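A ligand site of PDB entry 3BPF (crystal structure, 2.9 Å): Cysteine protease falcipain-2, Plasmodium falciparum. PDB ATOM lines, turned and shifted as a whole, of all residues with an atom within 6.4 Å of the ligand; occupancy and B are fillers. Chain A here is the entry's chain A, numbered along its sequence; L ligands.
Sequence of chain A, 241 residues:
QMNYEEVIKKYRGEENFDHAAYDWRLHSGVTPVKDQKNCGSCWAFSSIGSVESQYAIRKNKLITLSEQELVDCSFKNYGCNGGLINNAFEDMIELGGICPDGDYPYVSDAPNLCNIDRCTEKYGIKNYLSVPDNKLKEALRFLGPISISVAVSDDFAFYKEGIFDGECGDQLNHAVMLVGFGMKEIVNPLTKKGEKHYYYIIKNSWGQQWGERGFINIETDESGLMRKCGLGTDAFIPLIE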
ATOM      1  N   GLN A  36      -9.273  19.878 -15.043  1.00  0.00           N
ATOM      2  CA  GLN A  36      -9.646  20.325 -16.366  1.00  0.00           C
ATOM      3  C   GLN A  36      -8.718  21.462 -16.867  1.00  0.00           C
ATOM      4  O   GLN A  36      -8.869  21.969 -17.990  1.00  0.00           O
ATOM      5  CB  GLN A  36     -11.111  20.784 -16.356  1.00  0.00           C
ATOM      6  CG  GLN A  36     -11.329  22.164 -15.780  1.00  0.00           C
ATOM      7  CD  GLN A  36     -12.673  22.299 -15.147  1.00  0.00           C
ATOM      8  OE1 GLN A  36     -12.956  21.656 -14.150  1.00  0.00           O
ATOM      9  NE2 GLN A  36     -13.521  23.175 -15.702  1.00  0.00           N
ATOM     10  N   CYS A  39      -9.994  25.291 -19.750  1.00  0.00           N
ATOM     11  CA  CYS A  39     -10.810  24.518 -20.700  1.00  0.00           C
ATOM     12  C   CYS A  39     -12.171  24.276 -20.052  1.00  0.00           C
ATOM     13  O   CYS A  39     -12.277  23.432 -19.152  1.00  0.00           O
ATOM     14  CB  CYS A  39     -10.153  23.166 -21.037  1.00  0.00           C
ATOM     15  SG  CYS A  39     -11.166  22.009 -21.985  1.00  0.00           S
ATOM     16  N   GLY A  40     -13.191  25.006 -20.489  1.00  0.00           N
ATOM     17  CA  GLY A  40     -14.487  24.987 -19.809  1.00  0.00           C
ATOM     18  C   GLY A  40     -15.260  23.700 -19.986  1.00  0.00           C
ATOM     19  O   GLY A  40     -16.269  23.648 -20.680  1.00  0.00           O
ATOM     20  N   SER A  41     -14.789  22.659 -19.312  1.00  0.00           N
ATOM     21  CA  SER A  41     -15.290  21.330 -19.566  1.00  0.00           C
ATOM     22  C   SER A  41     -15.628  20.628 -18.262  1.00  0.00           C
ATOM     23  O   SER A  41     -15.327  19.437 -18.093  1.00  0.00           O
ATOM     24  CB  SER A  41     -14.255  20.533 -20.366  1.00  0.00           C
ATOM     25  OG  SER A  41     -13.036  20.383 -19.651  1.00  0.00           O
ATOM     26  N   CYS A  42     -16.273  21.344 -17.339  1.00  0.00           N
ATOM     27  CA  CYS A  42     -16.658  20.702 -16.091  1.00  0.00           C
ATOM     28  C   CYS A  42     -17.678  19.630 -16.396  1.00  0.00           C
ATOM     29  O   CYS A  42     -17.491  18.457 -16.035  1.00  0.00           O
ATOM     30  CB  CYS A  42     -17.227  21.707 -15.117  1.00  0.00           C
ATOM     31  SG  CYS A  42     -18.430  22.711 -15.900  1.00  0.00           S
ATOM     32  N   TRP A  43     -18.729  20.029 -17.119  1.00  0.00           N
ATOM     33  CA  TRP A  43     -19.747  19.111 -17.616  1.00  0.00           C
ATOM     34  C   TRP A  43     -19.190  17.761 -18.094  1.00  0.00           C
ATOM     35  O   TRP A  43     -19.824  16.724 -17.925  1.00  0.00           O
ATOM     36  CB  TRP A  43     -20.524  19.764 -18.760  1.00  0.00           C
ATOM     37  CG  TRP A  43     -19.669  20.017 -19.961  1.00  0.00           C
ATOM     38  CD1 TRP A  43     -18.927  21.114 -20.212  1.00  0.00           C
ATOM     39  CD2 TRP A  43     -19.464  19.134 -21.061  1.00  0.00           C
ATOM     40  NE1 TRP A  43     -18.276  20.979 -21.400  1.00  0.00           N
ATOM     41  CE2 TRP A  43     -18.582  19.768 -21.945  1.00  0.00           C
ATOM     42  CE3 TRP A  43     -19.934  17.849 -21.388  1.00  0.00           C
ATOM     43  CZ2 TRP A  43     -18.165  19.171 -23.138  1.00  0.00           C
ATOM     44  CZ3 TRP A  43     -19.519  17.262 -22.560  1.00  0.00           C
ATOM     45  CH2 TRP A  43     -18.636  17.928 -23.425  1.00  0.00           C
ATOM     46  N   TYR A  78     -20.481  22.097 -26.155  1.00  0.00           N
ATOM     47  CA  TYR A  78     -19.623  23.076 -26.828  1.00  0.00           C
ATOM     48  C   TYR A  78     -18.158  22.964 -26.389  1.00  0.00           C
ATOM     49  O   TYR A  78     -17.489  23.981 -26.169  1.00  0.00           O
ATOM     50  CB  TYR A  78     -20.179  24.454 -26.561  1.00  0.00           C
ATOM     51  CG  TYR A  78     -21.574  24.645 -27.089  1.00  0.00           C
ATOM     52  CD1 TYR A  78     -21.795  25.195 -28.346  1.00  0.00           C
ATOM     53  CD2 TYR A  78     -22.687  24.273 -26.334  1.00  0.00           C
ATOM     54  CE1 TYR A  78     -23.079  25.381 -28.844  1.00  0.00           C
ATOM     55  CE2 TYR A  78     -23.980  24.456 -26.821  1.00  0.00           C
ATOM     56  CZ  TYR A  78     -24.170  25.007 -28.082  1.00  0.00           C
ATOM     57  OH  TYR A  78     -25.439  25.209 -28.591  1.00  0.00           O
ATOM     58  N   GLY A  79     -17.666  21.734 -26.268  1.00  0.00           N
ATOM     59  CA  GLY A  79     -16.304  21.491 -25.818  1.00  0.00           C
ATOM     60  C   GLY A  79     -15.936  22.443 -24.694  1.00  0.00           C
ATOM     61  O   GLY A  79     -16.695  22.580 -23.736  1.00  0.00           O
ATOM     62  N   CYS A  80     -14.810  23.141 -24.840  1.00  0.00           N
ATOM     63  CA  CYS A  80     -14.336  24.069 -23.797  1.00  0.00           C
ATOM     64  C   CYS A  80     -15.218  25.316 -23.628  1.00  0.00           C
ATOM     65  O   CYS A  80     -15.058  26.053 -22.664  1.00  0.00           O
ATOM     66  CB  CYS A  80     -12.891  24.487 -24.052  1.00  0.00           C
ATOM     67  SG  CYS A  80     -11.714  23.238 -23.527  1.00  0.00           S
ATOM     68  N   ASN A  81     -16.149  25.560 -24.533  1.00  0.00           N
ATOM     69  CA  ASN A  81     -17.025  26.703 -24.344  1.00  0.00           C
ATOM     70  C   ASN A  81     -18.292  26.362 -23.533  1.00  0.00           C
ATOM     71  O   ASN A  81     -19.216  27.194 -23.408  1.00  0.00           O
ATOM     72  CB  ASN A  81     -17.351  27.347 -25.682  1.00  0.00           C
ATOM     73  CG  ASN A  81     -16.124  27.976 -26.329  1.00  0.00           C
ATOM     74  OD1 ASN A  81     -15.969  29.193 -26.312  1.00  0.00           O
ATOM     75  ND2 ASN A  81     -15.255  27.148 -26.882  1.00  0.00           N
ATOM     76  N   GLY A  82     -18.314  25.144 -22.971  1.00  0.00           N
ATOM     77  CA  GLY A  82     -19.334  24.746 -22.014  1.00  0.00           C
ATOM     78  C   GLY A  82     -20.016  23.431 -22.330  1.00  0.00           C
ATOM     79  O   GLY A  82     -19.513  22.664 -23.138  1.00  0.00           O
ATOM     80  N   GLY A  83     -21.154  23.192 -21.674  1.00  0.00           N
ATOM     81  CA  GLY A  83     -21.939  21.965 -21.870  1.00  0.00           C
ATOM     82  C   GLY A  83     -22.939  21.676 -20.755  1.00  0.00           C
ATOM     83  O   GLY A  83     -23.025  22.424 -19.777  1.00  0.00           O
ATOM     84  N   LEU A  84     -23.706  20.592 -20.914  1.00  0.00           N
ATOM     85  CA  LEU A  84     -24.693  20.172 -19.910  1.00  0.00           C
ATOM     86  C   LEU A  84     -24.561  18.686 -19.592  1.00  0.00           C
ATOM     87  O   LEU A  84     -24.250  17.875 -20.451  1.00  0.00           O
ATOM     88  CB  LEU A  84     -26.116  20.458 -20.395  1.00  0.00           C
ATOM     89  CG  LEU A  84     -26.488  21.904 -20.699  1.00  0.00           C
ATOM     90  CD1 LEU A  84     -27.903  21.972 -21.214  1.00  0.00           C
ATOM     91  CD2 LEU A  84     -26.334  22.770 -19.464  1.00  0.00           C
ATOM     92  N   ILE A  85     -24.850  18.351 -18.335  1.00  0.00           N
ATOM     93  CA  ILE A  85     -24.598  17.007 -17.809  1.00  0.00           C
ATOM     94  C   ILE A  85     -25.433  16.001 -18.585  1.00  0.00           C
ATOM     95  O   ILE A  85     -24.886  15.051 -19.165  1.00  0.00           O
ATOM     96  CB  ILE A  85     -24.915  16.920 -16.300  1.00  0.00           C
ATOM     97  CG1 ILE A  85     -24.050  17.904 -15.507  1.00  0.00           C
ATOM     98  CG2 ILE A  85     -24.697  15.521 -15.770  1.00  0.00           C
ATOM     99  CD1 ILE A  85     -24.509  18.078 -14.087  1.00  0.00           C
ATOM    100  N   ILE A 148     -23.707  16.894 -10.611  1.00  0.00           N
ATOM    101  CA  ILE A 148     -24.619  17.965 -10.176  1.00  0.00           C
ATOM    102  C   ILE A 148     -24.117  19.382 -10.456  1.00  0.00           C
ATOM    103  O   ILE A 148     -22.940  19.600 -10.573  1.00  0.00           O
ATOM    104  CB  ILE A 148     -24.924  17.840  -8.668  1.00  0.00           C
ATOM    105  CG1 ILE A 148     -23.674  18.130  -7.818  1.00  0.00           C
ATOM    106  CG2 ILE A 148     -25.432  16.429  -8.328  1.00  0.00           C
ATOM    107  CD1 ILE A 148     -23.990  18.993  -6.617  1.00  0.00           C
ATOM    108  N   SER A 149     -25.025  20.353 -10.534  1.00  0.00           N
ATOM    109  CA  SER A 149     -24.641  21.750 -10.791  1.00  0.00           C
ATOM    110  C   SER A 149     -24.323  22.469  -9.481  1.00  0.00           C
ATOM    111  O   SER A 149     -24.487  21.875  -8.406  1.00  0.00           O
ATOM    112  CB  SER A 149     -25.744  22.503 -11.552  1.00  0.00           C
ATOM    113  OG  SER A 149     -26.988  22.458 -10.867  1.00  0.00           O
ATOM    114  N   VAL A 150     -23.866  23.729  -9.584  1.00  0.00           N
ATOM    115  CA  VAL A 150     -23.587  24.585  -8.411  1.00  0.00           C
ATOM    116  C   VAL A 150     -23.059  25.952  -8.814  1.00  0.00           C
ATOM    117  O   VAL A 150     -22.233  26.070  -9.709  1.00  0.00           O
ATOM    118  CB  VAL A 150     -22.536  23.979  -7.445  1.00  0.00           C
ATOM    119  CG1 VAL A 150     -21.256  23.602  -8.172  1.00  0.00           C
ATOM    120  CG2 VAL A 150     -22.248  24.956  -6.294  1.00  0.00           C
ATOM    121  N   GLN A 171     -25.222  32.586 -10.553  1.00  0.00           N
ATOM    122  CA  GLN A 171     -26.110  31.643 -11.213  1.00  0.00           C
ATOM    123  C   GLN A 171     -25.484  30.259 -11.125  1.00  0.00           C
ATOM    124  O   GLN A 171     -24.284  30.156 -10.851  1.00  0.00           O
ATOM    125  CB  GLN A 171     -26.281  32.016 -12.686  1.00  0.00           C
ATOM    126  CG  GLN A 171     -24.977  31.842 -13.526  1.00  0.00           C
ATOM    127  CD  GLN A 171     -25.219  31.917 -15.041  1.00  0.00           C
ATOM    128  OE1 GLN A 171     -26.044  32.715 -15.527  1.00  0.00           O
ATOM    129  NE2 GLN A 171     -24.468  31.095 -15.792  1.00  0.00           N
ATOM    130  N   LEU A 172     -26.253  29.209 -11.394  1.00  0.00           N
ATOM    131  CA  LEU A 172     -25.652  27.886 -11.556  1.00  0.00           C
ATOM    132  C   LEU A 172     -24.608  28.021 -12.654  1.00  0.00           C
ATOM    133  O   LEU A 172     -24.938  28.467 -13.770  1.00  0.00           O
ATOM    134  CB  LEU A 172     -26.686  26.833 -11.929  1.00  0.00           C
ATOM    135  CG  LEU A 172     -27.479  26.201 -10.792  1.00  0.00           C
ATOM    136  CD1 LEU A 172     -28.578  25.310 -11.362  1.00  0.00           C
ATOM    137  CD2 LEU A 172     -26.540  25.410  -9.885  1.00  0.00           C
ATOM    138  N   ASN A 173     -23.364  27.678 -12.352  1.00  0.00           N
ATOM    139  CA  ASN A 173     -22.262  27.944 -13.266  1.00  0.00           C
ATOM    140  C   ASN A 173     -21.171  26.874 -13.396  1.00  0.00           C
ATOM    141  O   ASN A 173     -20.188  27.092 -14.077  1.00  0.00           O
ATOM    142  CB  ASN A 173     -21.613  29.300 -12.926  1.00  0.00           C
ATOM    143  CG  ASN A 173     -20.914  29.302 -11.568  1.00  0.00           C
ATOM    144  OD1 ASN A 173     -20.493  28.269 -11.050  1.00  0.00           O
ATOM    145  ND2 ASN A 173     -20.787  30.483 -10.995  1.00  0.00           N
ATOM    146  N   HIS A 174     -21.345  25.718 -12.769  1.00  0.00           N
ATOM    147  CA  HIS A 174     -20.259  24.756 -12.678  1.00  0.00           C
ATOM    148  C   HIS A 174     -20.793  23.347 -12.376  1.00  0.00           C
ATOM    149  O   HIS A 174     -21.874  23.194 -11.816  1.00  0.00           O
ATOM    150  CB  HIS A 174     -19.241  25.224 -11.616  1.00  0.00           C
ATOM    151  CG  HIS A 174     -18.003  24.400 -11.551  1.00  0.00           C
ATOM    152  ND1 HIS A 174     -17.117  24.299 -12.603  1.00  0.00           N
ATOM    153  CD2 HIS A 174     -17.500  23.604 -10.561  1.00  0.00           C
ATOM    154  CE1 HIS A 174     -16.139  23.473 -12.271  1.00  0.00           C
ATOM    155  NE2 HIS A 174     -16.343  23.041 -11.033  1.00  0.00           N
ATOM    156  N   ALA A 175     -20.045  22.325 -12.784  1.00  0.00           N
ATOM    157  CA  ALA A 175     -20.435  20.937 -12.566  1.00  0.00           C
ATOM    158  C   ALA A 175     -19.487  20.326 -11.580  1.00  0.00           C
ATOM    159  O   ALA A 175     -18.294  20.652 -11.599  1.00  0.00           O
ATOM    160  CB  ALA A 175     -20.383  20.165 -13.863  1.00  0.00           C
ATOM    161  N   SER A 205     -13.120  19.291 -10.180  1.00  0.00           N
ATOM    162  CA  SER A 205     -12.304  18.958 -11.353  1.00  0.00           C
ATOM    163  C   SER A 205     -11.215  19.993 -11.547  1.00  0.00           C
ATOM    164  O   SER A 205     -10.885  20.339 -12.677  1.00  0.00           O
ATOM    165  CB  SER A 205     -13.185  18.870 -12.592  1.00  0.00           C
ATOM    166  OG  SER A 205     -14.016  20.015 -12.689  1.00  0.00           O
ATOM    167  N   TRP A 206     -10.656  20.483 -10.430  1.00  0.00           N
ATOM    168  CA  TRP A 206      -9.639  21.531 -10.456  1.00  0.00           C
ATOM    169  C   TRP A 206      -8.291  21.039  -9.952  1.00  0.00           C
ATOM    170  O   TRP A 206      -7.453  21.834  -9.557  1.00  0.00           O
ATOM    171  CB  TRP A 206     -10.075  22.701  -9.597  1.00  0.00           C
ATOM    172  CG  TRP A 206     -11.236  23.416 -10.120  1.00  0.00           C
ATOM    173  CD1 TRP A 206     -11.810  23.274 -11.349  1.00  0.00           C
ATOM    174  CD2 TRP A 206     -11.953  24.453  -9.454  1.00  0.00           C
ATOM    175  NE1 TRP A 206     -12.864  24.164 -11.472  1.00  0.00           N
ATOM    176  CE2 TRP A 206     -12.959  24.893 -10.332  1.00  0.00           C
ATOM    177  CE3 TRP A 206     -11.833  25.052  -8.203  1.00  0.00           C
ATOM    178  CZ2 TRP A 206     -13.866  25.894  -9.978  1.00  0.00           C
ATOM    179  CZ3 TRP A 206     -12.731  26.057  -7.860  1.00  0.00           C
ATOM    180  CH2 TRP A 206     -13.734  26.456  -8.749  1.00  0.00           C
ATOM    181  N   ASP A 234     -29.603  20.886 -10.569  1.00  0.00           N
ATOM    182  CA  ASP A 234     -29.499  19.806 -11.557  1.00  0.00           C
ATOM    183  C   ASP A 234     -28.748  18.651 -10.920  1.00  0.00           C
ATOM    184  O   ASP A 234     -27.708  18.842 -10.280  1.00  0.00           O
ATOM    185  CB  ASP A 234     -28.747  20.257 -12.790  1.00  0.00           C
ATOM    186  CG  ASP A 234     -29.215  21.590 -13.275  1.00  0.00           C
ATOM    187  OD1 ASP A 234     -30.408  21.718 -13.600  1.00  0.00           O
ATOM    188  OD2 ASP A 234     -28.379  22.513 -13.303  1.00  0.00           O
HETATM  189  C1  LIG L   1     -16.649  24.839 -16.028  1.00  0.00           C
HETATM  190  O1  LIG L   1     -16.619  25.811 -15.234  1.00  0.00           O
HETATM  191  O2  LIG L   1     -15.664  24.227 -16.483  1.00  0.00           O
HETATM  192  C2  LIG L   1     -18.029  24.366 -16.472  1.00  0.00           C
HETATM  193  C3  LIG L   1     -18.346  24.836 -17.901  1.00  0.00           C
HETATM  194  O3  LIG L   1     -18.103  26.223 -18.004  1.00  0.00           O
HETATM  195  C4  LIG L   1     -19.821  24.569 -18.166  1.00  0.00           C
HETATM  196  O4  LIG L   1     -20.188  23.855 -19.090  1.00  0.00           O
HETATM  197  N1  LIG L   1     -20.637  25.176 -17.317  1.00  0.00           N
HETATM  198  C5  LIG L   1     -22.102  25.024 -17.403  1.00  0.00           C
HETATM  199  C6  LIG L   1     -22.710  25.391 -16.049  1.00  0.00           C
HETATM  200  C7  LIG L   1     -23.724  24.333 -15.611  1.00  0.00           C
HETATM  201  C8  LIG L   1     -23.130  22.910 -15.660  1.00  0.00           C
HETATM  202  C9  LIG L   1     -24.270  24.689 -14.213  1.00  0.00           C
HETATM  203  C10 LIG L   1     -22.647  25.945 -18.480  1.00  0.00           C
HETATM  204  O5  LIG L   1     -22.458  27.162 -18.437  1.00  0.00           O
HETATM  205  N2  LIG L   1     -23.313  25.319 -19.436  1.00  0.00           N
HETATM  206  C11 LIG L   1     -23.924  26.018 -20.576  1.00  0.00           C
HETATM  207  C12 LIG L   1     -22.892  26.181 -21.693  1.00  0.00           C
HETATM  208  C13 LIG L   1     -23.531  25.968 -23.076  1.00  0.00           C
HETATM  209  C14 LIG L   1     -23.874  27.317 -23.745  1.00  0.00           C
HETATM  210  N3  LIG L   1     -22.636  28.037 -24.072  1.00  0.00           N
HETATM  211  C15 LIG L   1     -22.170  28.168 -25.324  1.00  0.00           C
HETATM  212  N4  LIG L   1     -22.818  27.624 -26.352  1.00  0.00           N
HETATM  213  N5  LIG L   1     -21.039  28.827 -25.550  1.00  0.00           N
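The side-chain hydroxyl (OG) of Ser 149 lies within hydrogen-bond range of the side-chain carboxylate (OD2) of Asp 234, 2.8 Å away.
The side-chain amide oxygen (OD1) of Asn 173 sits close to the backbone carbonyl oxygen (O) of Val 150 (3.1 Å).
O of His 174 lies within hydrogen-bond range of N of Val 150 (3.0 Å).
OE1 of Gln 36 sits at hydrogen-bond distance from OG of Ser 205 (2.4 Å).
The backbone carbonyl oxygen of Gly 40 sits at hydrogen-bond distance from the indole nitrogen of Trp 43 (3.4 Å).
The backbone NH (N) of Ala 175 lies within hydrogen-bond range of the side-chain sulfur (SG) of Cys 42 (3.5 Å).
SG of Cys 39 forms a disulfide with SG of Cys 80.
The indole nitrogen (NE1) of Trp 43 lies within hydrogen-bond range of the backbone carbonyl oxygen (O) of Gly 79 (3.2 Å).
Gly 40 touches the ligand.
CD1 of Trp 43 touches O4 of the ligand (3.2 Å).
CD1 of Tyr 78 touches N4 of the ligand (3.3 Å).
Gly 82 touches the ligand (CA to O4, 3.2 Å).
Leu 84 touches the ligand.
Ser 149 touches the ligand (CB to C9, 3.7 Å).
Leu 172 touches the ligand (C to C9, 3.7 Å).
Asn 173 touches the ligand.
Hydrophobic or aromatic side chains that line the ligand: Trp 43, Tyr 78, Leu 84, Leu 172 and His 174.
14 residues have an atom within 4 Å of the ligand: Gln 36, Gly 40, Ser 41, Cys 42, Trp 43, Tyr 78, Asn 81, Gly 82, Gly 83, Leu 84, Ser 149, Leu 172, Asn 173 and His 174.
Along chain A the residues within 4 Å of the ligand span positions 36 to 174.
The nearest printed residue that does not touch the ligand is Ala 175 (4.3 Å).
ND1 of His 174 is in hydrogen-bond range of O1 of the ligand (3.1 Å).
The backbone NH of Cys 42 lies within hydrogen-bond range of an oxygen (O2) of the ligand, at 3.1 Å.
An oxygen (O2) of the ligand sits at hydrogen-bond distance from the backbone NH of Ser 41.
The side-chain amide nitrogen (NE2) of Gln 36 lies within hydrogen-bond range of an oxygen (O2) of the ligand (2.5 Å).
O of Asn 81 sits at hydrogen-bond distance from N5 of the ligand (3.3 Å).
SG of Cys 42 is covalently linked to C2 of the ligand.
The backbone NH of Gly 83 lies within hydrogen-bond range of an oxygen (O4) of the ligand, at 2.8 Å.
The backbone carbonyl oxygen (O) of Gly 83 sits at hydrogen-bond distance from a nitrogen (N2) of the ligand.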
